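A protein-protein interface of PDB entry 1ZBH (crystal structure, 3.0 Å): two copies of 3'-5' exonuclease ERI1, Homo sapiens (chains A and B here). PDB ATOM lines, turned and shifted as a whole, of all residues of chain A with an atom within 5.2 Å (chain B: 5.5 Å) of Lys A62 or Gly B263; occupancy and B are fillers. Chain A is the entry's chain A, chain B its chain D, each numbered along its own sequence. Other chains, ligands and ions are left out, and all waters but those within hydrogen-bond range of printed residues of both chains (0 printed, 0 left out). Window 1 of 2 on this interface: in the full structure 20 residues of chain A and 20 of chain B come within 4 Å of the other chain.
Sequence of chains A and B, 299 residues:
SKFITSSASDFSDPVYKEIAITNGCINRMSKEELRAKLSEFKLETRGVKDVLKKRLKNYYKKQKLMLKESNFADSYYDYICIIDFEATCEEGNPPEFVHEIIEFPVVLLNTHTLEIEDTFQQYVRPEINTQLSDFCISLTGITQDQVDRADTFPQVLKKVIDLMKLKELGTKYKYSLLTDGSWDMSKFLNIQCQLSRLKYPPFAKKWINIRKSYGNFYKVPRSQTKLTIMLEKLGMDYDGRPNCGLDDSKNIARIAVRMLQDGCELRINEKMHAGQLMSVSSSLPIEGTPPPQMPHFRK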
ATOM      1  N   ASN A  58     -27.464  27.045  15.840  1.00  0.00           N
ATOM      2  CA  ASN A  58     -27.612  26.138  14.702  1.00  0.00           C
ATOM      3  C   ASN A  58     -28.553  24.967  14.957  1.00  0.00           C
ATOM      4  O   ASN A  58     -29.227  24.503  14.037  1.00  0.00           O
ATOM      5  CB  ASN A  58     -26.250  25.618  14.236  1.00  0.00           C
ATOM      6  CG  ASN A  58     -25.648  26.462  13.125  1.00  0.00           C
ATOM      7  OD1 ASN A  58     -25.624  27.692  13.201  1.00  0.00           O
ATOM      8  ND2 ASN A  58     -25.151  25.799  12.086  1.00  0.00           N
ATOM      9  N   TYR A  59     -28.597  24.490  16.198  1.00  0.00           N
ATOM     10  CA  TYR A  59     -29.499  23.398  16.555  1.00  0.00           C
ATOM     11  C   TYR A  59     -30.967  23.821  16.470  1.00  0.00           C
ATOM     12  O   TYR A  59     -31.796  23.076  15.943  1.00  0.00           O
ATOM     13  CB  TYR A  59     -29.174  22.833  17.941  1.00  0.00           C
ATOM     14  CG  TYR A  59     -30.063  21.676  18.341  1.00  0.00           C
ATOM     15  CD1 TYR A  59     -29.846  20.395  17.829  1.00  0.00           C
ATOM     16  CD2 TYR A  59     -31.128  21.863  19.223  1.00  0.00           C
ATOM     17  CE1 TYR A  59     -30.665  19.331  18.188  1.00  0.00           C
ATOM     18  CE2 TYR A  59     -31.953  20.807  19.587  1.00  0.00           C
ATOM     19  CZ  TYR A  59     -31.715  19.545  19.068  1.00  0.00           C
ATOM     20  OH  TYR A  59     -32.527  18.497  19.429  1.00  0.00           O
ATOM     21  N   TYR A  60     -31.278  25.010  16.986  1.00  0.00           N
ATOM     22  CA  TYR A  60     -32.628  25.577  16.890  1.00  0.00           C
ATOM     23  C   TYR A  60     -33.005  25.919  15.448  1.00  0.00           C
ATOM     24  O   TYR A  60     -34.188  26.025  15.117  1.00  0.00           O
ATOM     25  CB  TYR A  60     -32.779  26.811  17.790  1.00  0.00           C
ATOM     26  CG  TYR A  60     -33.218  26.498  19.208  1.00  0.00           C
ATOM     27  CD1 TYR A  60     -34.569  26.317  19.518  1.00  0.00           C
ATOM     28  CD2 TYR A  60     -32.286  26.387  20.239  1.00  0.00           C
ATOM     29  CE1 TYR A  60     -34.978  26.028  20.819  1.00  0.00           C
ATOM     30  CE2 TYR A  60     -32.685  26.100  21.544  1.00  0.00           C
ATOM     31  CZ  TYR A  60     -34.030  25.922  21.826  1.00  0.00           C
ATOM     32  OH  TYR A  60     -34.426  25.638  23.114  1.00  0.00           O
ATOM     33  N   LYS A  61     -31.993  26.093  14.600  1.00  0.00           N
ATOM     34  CA  LYS A  61     -32.198  26.316  13.174  1.00  0.00           C
ATOM     35  C   LYS A  61     -32.404  24.986  12.441  1.00  0.00           C
ATOM     36  O   LYS A  61     -33.254  24.886  11.555  1.00  0.00           O
ATOM     37  CB  LYS A  61     -31.021  27.091  12.576  1.00  0.00           C
ATOM     38  CG  LYS A  61     -31.283  27.646  11.185  1.00  0.00           C
ATOM     39  CD  LYS A  61     -30.034  28.276  10.593  1.00  0.00           C
ATOM     40  CE  LYS A  61     -30.261  28.673   9.144  1.00  0.00           C
ATOM     41  NZ  LYS A  61     -29.103  29.420   8.589  1.00  0.00           N
ATOM     42  N   LYS A  62     -31.629  23.972  12.819  1.00  0.00           N
ATOM     43  CA  LYS A  62     -31.765  22.632  12.246  1.00  0.00           C
ATOM     44  C   LYS A  62     -32.983  21.878  12.773  1.00  0.00           C
ATOM     45  O   LYS A  62     -33.319  20.813  12.258  1.00  0.00           O
ATOM     46  CB  LYS A  62     -30.497  21.800  12.474  1.00  0.00           C
ATOM     47  CG  LYS A  62     -29.572  21.700  11.263  1.00  0.00           C
ATOM     48  CD  LYS A  62     -28.578  22.855  11.195  1.00  0.00           C
ATOM     49  CE  LYS A  62     -27.617  22.700  10.026  1.00  0.00           C
ATOM     50  NZ  LYS A  62     -26.735  21.508  10.163  1.00  0.00           N
ATOM     51  N   GLN A  63     -33.633  22.424  13.799  1.00  0.00           N
ATOM     52  CA  GLN A  63     -34.843  21.818  14.361  1.00  0.00           C
ATOM     53  C   GLN A  63     -36.128  22.457  13.832  1.00  0.00           C
ATOM     54  O   GLN A  63     -37.074  21.751  13.481  1.00  0.00           O
ATOM     55  CB  GLN A  63     -34.819  21.858  15.892  1.00  0.00           C
ATOM     56  CG  GLN A  63     -34.083  20.689  16.539  1.00  0.00           C
ATOM     57  CD  GLN A  63     -34.796  19.356  16.354  1.00  0.00           C
ATOM     58  OE1 GLN A  63     -34.168  18.345  16.047  1.00  0.00           O
ATOM     59  NE2 GLN A  63     -36.114  19.352  16.538  1.00  0.00           N
ATOM     60  N   LYS A  64     -36.149  23.787  13.776  1.00  0.00           N
ATOM     61  CA  LYS A  64     -37.327  24.532  13.323  1.00  0.00           C
ATOM     62  C   LYS A  64     -37.525  24.480  11.807  1.00  0.00           C
ATOM     63  O   LYS A  64     -38.657  24.544  11.329  1.00  0.00           O
ATOM     64  CB  LYS A  64     -37.285  25.982  13.818  1.00  0.00           C
ATOM     65  CG  LYS A  64     -37.587  26.128  15.305  1.00  0.00           C
ATOM     66  CD  LYS A  64     -37.600  27.580  15.750  1.00  0.00           C
ATOM     67  CE  LYS A  64     -37.962  27.689  17.226  1.00  0.00           C
ATOM     68  NZ  LYS A  64     -38.078  29.099  17.684  1.00  0.00           N
ATOM     69  N   LEU A  65     -36.426  24.366  11.061  1.00  0.00           N
ATOM     70  CA  LEU A  65     -36.490  24.204   9.607  1.00  0.00           C
ATOM     71  C   LEU A  65     -36.743  22.753   9.210  1.00  0.00           C
ATOM     72  O   LEU A  65     -37.273  22.485   8.132  1.00  0.00           O
ATOM     73  CB  LEU A  65     -35.218  24.726   8.929  1.00  0.00           C
ATOM     74  CG  LEU A  65     -35.065  26.239   8.736  1.00  0.00           C
ATOM     75  CD1 LEU A  65     -33.636  26.585   8.347  1.00  0.00           C
ATOM     76  CD2 LEU A  65     -36.044  26.780   7.699  1.00  0.00           C
ATOM     77  N   MET A  66     -36.357  21.825  10.083  1.00  0.00           N
ATOM     78  CA  MET A  66     -36.599  20.401   9.871  1.00  0.00           C
ATOM     79  C   MET A  66     -38.044  20.045  10.206  1.00  0.00           C
ATOM     80  O   MET A  66     -38.670  19.249   9.504  1.00  0.00           O
ATOM     81  CB  MET A  66     -35.641  19.567  10.722  1.00  0.00           C
ATOM     82  CG  MET A  66     -35.585  18.089  10.365  1.00  0.00           C
ATOM     83  SD  MET A  66     -34.628  17.122  11.552  1.00  0.00           S
ATOM     84  CE  MET A  66     -32.953  17.648  11.188  1.00  0.00           C
ATOM     85  N   PHE B  72     -27.275  16.135   7.094  1.00  0.00           N
ATOM     86  CA  PHE B  72     -27.015  16.848   8.350  1.00  0.00           C
ATOM     87  C   PHE B  72     -25.667  16.432   8.946  1.00  0.00           C
ATOM     88  O   PHE B  72     -25.405  15.236   9.138  1.00  0.00           O
ATOM     89  CB  PHE B  72     -28.164  16.640   9.350  1.00  0.00           C
ATOM     90  CG  PHE B  72     -29.529  16.955   8.783  1.00  0.00           C
ATOM     91  CD1 PHE B  72     -30.397  15.925   8.408  1.00  0.00           C
ATOM     92  CD2 PHE B  72     -29.942  18.280   8.608  1.00  0.00           C
ATOM     93  CE1 PHE B  72     -31.659  16.210   7.872  1.00  0.00           C
ATOM     94  CE2 PHE B  72     -31.203  18.577   8.071  1.00  0.00           C
ATOM     95  CZ  PHE B  72     -32.063  17.540   7.702  1.00  0.00           C
ATOM     96  N   ALA B  73     -24.829  17.433   9.235  1.00  0.00           N
ATOM     97  CA  ALA B  73     -23.413  17.248   9.606  1.00  0.00           C
ATOM     98  C   ALA B  73     -22.559  16.727   8.434  1.00  0.00           C
ATOM     99  O   ALA B  73     -21.399  16.335   8.615  1.00  0.00           O
ATOM    100  CB  ALA B  73     -23.265  16.360  10.859  1.00  0.00           C
ATOM    101  N   PHE B 217     -18.151  32.347  10.808  1.00  0.00           N
ATOM    102  CA  PHE B 217     -19.084  31.380  11.379  1.00  0.00           C
ATOM    103  C   PHE B 217     -19.231  31.643  12.876  1.00  0.00           C
ATOM    104  O   PHE B 217     -20.340  31.859  13.367  1.00  0.00           O
ATOM    105  CB  PHE B 217     -18.626  29.944  11.122  1.00  0.00           C
ATOM    106  CG  PHE B 217     -19.591  28.900  11.611  1.00  0.00           C
ATOM    107  CD1 PHE B 217     -20.767  28.640  10.914  1.00  0.00           C
ATOM    108  CD2 PHE B 217     -19.319  28.171  12.762  1.00  0.00           C
ATOM    109  CE1 PHE B 217     -21.660  27.673  11.362  1.00  0.00           C
ATOM    110  CE2 PHE B 217     -20.205  27.202  13.217  1.00  0.00           C
ATOM    111  CZ  PHE B 217     -21.378  26.951  12.515  1.00  0.00           C
ATOM    112  N   ARG B 258     -15.327  19.658  13.833  1.00  0.00           N
ATOM    113  CA  ARG B 258     -16.090  20.388  14.842  1.00  0.00           C
ATOM    114  C   ARG B 258     -17.040  21.406  14.211  1.00  0.00           C
ATOM    115  O   ARG B 258     -18.152  21.619  14.700  1.00  0.00           O
ATOM    116  CB  ARG B 258     -15.128  21.081  15.815  1.00  0.00           C
ATOM    117  CG  ARG B 258     -15.782  21.880  16.944  1.00  0.00           C
ATOM    118  CD  ARG B 258     -16.344  20.987  18.045  1.00  0.00           C
ATOM    119  NE  ARG B 258     -17.648  20.428  17.690  1.00  0.00           N
ATOM    120  CZ  ARG B 258     -18.248  19.435  18.343  1.00  0.00           C
ATOM    121  NH1 ARG B 258     -19.432  19.000  17.938  1.00  0.00           N
ATOM    122  NH2 ARG B 258     -17.665  18.873  19.394  1.00  0.00           N
ATOM    123  N   MET B 259     -16.593  22.014  13.115  1.00  0.00           N
ATOM    124  CA  MET B 259     -17.371  23.020  12.402  1.00  0.00           C
ATOM    125  C   MET B 259     -18.504  22.410  11.581  1.00  0.00           C
ATOM    126  O   MET B 259     -19.611  22.946  11.566  1.00  0.00           O
ATOM    127  CB  MET B 259     -16.462  23.877  11.523  1.00  0.00           C
ATOM    128  CG  MET B 259     -15.593  24.840  12.316  1.00  0.00           C
ATOM    129  SD  MET B 259     -14.447  25.783  11.300  1.00  0.00           S
ATOM    130  CE  MET B 259     -15.578  26.805  10.359  1.00  0.00           C
ATOM    131  N   LEU B 260     -18.227  21.295  10.909  1.00  0.00           N
ATOM    132  CA  LEU B 260     -19.244  20.580  10.139  1.00  0.00           C
ATOM    133  C   LEU B 260     -20.306  19.989  11.058  1.00  0.00           C
ATOM    134  O   LEU B 260     -21.480  19.898  10.686  1.00  0.00           O
ATOM    135  CB  LEU B 260     -18.607  19.472   9.298  1.00  0.00           C
ATOM    136  CG  LEU B 260     -17.738  19.887   8.109  1.00  0.00           C
ATOM    137  CD1 LEU B 260     -16.791  18.760   7.721  1.00  0.00           C
ATOM    138  CD2 LEU B 260     -18.586  20.323   6.920  1.00  0.00           C
ATOM    139  N   GLN B 261     -19.875  19.583  12.253  1.00  0.00           N
ATOM    140  CA  GLN B 261     -20.771  19.093  13.298  1.00  0.00           C
ATOM    141  C   GLN B 261     -21.673  20.215  13.782  1.00  0.00           C
ATOM    142  O   GLN B 261     -22.878  20.026  13.933  1.00  0.00           O
ATOM    143  CB  GLN B 261     -19.975  18.521  14.473  1.00  0.00           C
ATOM    144  CG  GLN B 261     -19.359  17.163  14.193  1.00  0.00           C
ATOM    145  CD  GLN B 261     -18.366  16.718  15.251  1.00  0.00           C
ATOM    146  OE1 GLN B 261     -17.744  17.536  15.932  1.00  0.00           O
ATOM    147  NE2 GLN B 261     -18.202  15.408  15.382  1.00  0.00           N
ATOM    148  N   ASP B 262     -21.075  21.384  14.007  1.00  0.00           N
ATOM    149  CA  ASP B 262     -21.811  22.585  14.388  1.00  0.00           C
ATOM    150  C   ASP B 262     -22.709  23.081  13.255  1.00  0.00           C
ATOM    151  O   ASP B 262     -23.594  23.910  13.475  1.00  0.00           O
ATOM    152  CB  ASP B 262     -20.847  23.690  14.842  1.00  0.00           C
ATOM    153  CG  ASP B 262     -20.314  23.470  16.256  1.00  0.00           C
ATOM    154  OD1 ASP B 262     -19.554  24.334  16.742  1.00  0.00           O
ATOM    155  OD2 ASP B 262     -20.651  22.443  16.885  1.00  0.00           O
ATOM    156  N   GLY B 263     -22.477  22.570  12.048  1.00  0.00           N
ATOM    157  CA  GLY B 263     -23.335  22.857  10.904  1.00  0.00           C
ATOM    158  C   GLY B 263     -22.843  23.966   9.997  1.00  0.00           C
ATOM    159  O   GLY B 263     -23.644  24.641   9.348  1.00  0.00           O
ATOM    160  N   CYS B 264     -21.525  24.160   9.957  1.00  0.00           N
ATOM    161  CA  CYS B 264     -20.913  25.096   9.021  1.00  0.00           C
ATOM    162  C   CYS B 264     -20.790  24.425   7.668  1.00  0.00           C
ATOM    163  O   CYS B 264     -20.120  23.400   7.536  1.00  0.00           O
ATOM    164  CB  CYS B 264     -19.530  25.548   9.506  1.00  0.00           C
ATOM    165  SG  CYS B 264     -18.803  26.908   8.542  1.00  0.00           S
ATOM    166  N   GLU B 265     -21.456  24.993   6.670  1.00  0.00           N
ATOM    167  CA  GLU B 265     -21.316  24.527   5.299  1.00  0.00           C
ATOM    168  C   GLU B 265     -19.971  25.035   4.789  1.00  0.00           C
ATOM    169  O   GLU B 265     -19.896  26.099   4.172  1.00  0.00           O
ATOM    170  CB  GLU B 265     -22.463  25.045   4.418  1.00  0.00           C
ATOM    171  CG  GLU B 265     -23.879  24.902   5.009  1.00  0.00           C
ATOM    172  CD  GLU B 265     -24.490  23.512   4.831  1.00  0.00           C
ATOM    173  OE1 GLU B 265     -23.844  22.626   4.223  1.00  0.00           O
ATOM    174  OE2 GLU B 265     -25.631  23.310   5.302  1.00  0.00           O
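The side-chain amide nitrogen of Asn A58 sits at hydrogen-bond distance from the backbone carbonyl oxygen of Asp B262.
The side-chain amide nitrogen of Asn A58 sits at hydrogen-bond distance from the backbone carbonyl oxygen of Gly B263 (3.3 Å).
The side-chain carboxylate (OD2) of Asp B262 is in salt-bridge range of the guanidinium group (NE) of Arg B258 (3.7 Å).
ND2 of Asn A58 touches CZ of Phe B217 (3.97 Å).
Lys A62 touches Gly B263.
Met A66 touches Phe B72 (CE to CZ, 3.6 Å).
Lys A62 touches one residue of chain B.
Of chain A, only Asn A58 (3.3 Å) and Lys A62 (3.7 Å) come within 4 Å of Gly B263.
Printed residues of chain A within 4 Å of Phe B72: Met A66.
Of the printed residues of chain B, Asn A58 touches Phe B217 (3.97 Å), Asp B262 (2.8 Å) and Gly B263 (3.3 Å).
Printed residues of chain B within 4 Å of Met A66: Phe B72 (3.6 Å).
Printed residues of chain A within 4 Å of Asp B262: Asn A58 (2.8 Å).
The nearest residue of chain B that does not touch Lys A62 is Phe B72 (4.3 Å).
The nearest printed residue of chain A that does not touch Gly B263 is Lys A61 (7.3 Å).
Of the 9 printed residues of chain A, 3 touch a printed residue of chain B.
Hydrophobic or aromatic side chains of chain A that line the printed part of chain B: Met A66.
Of the 11 printed residues of chain B, 4 touch a printed residue of chain A.
Hydrophobic or aromatic side chains of chain B within 4 Å of the printed part of chain A: Phe B72 and Phe B217.
No position is printed for both chains.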
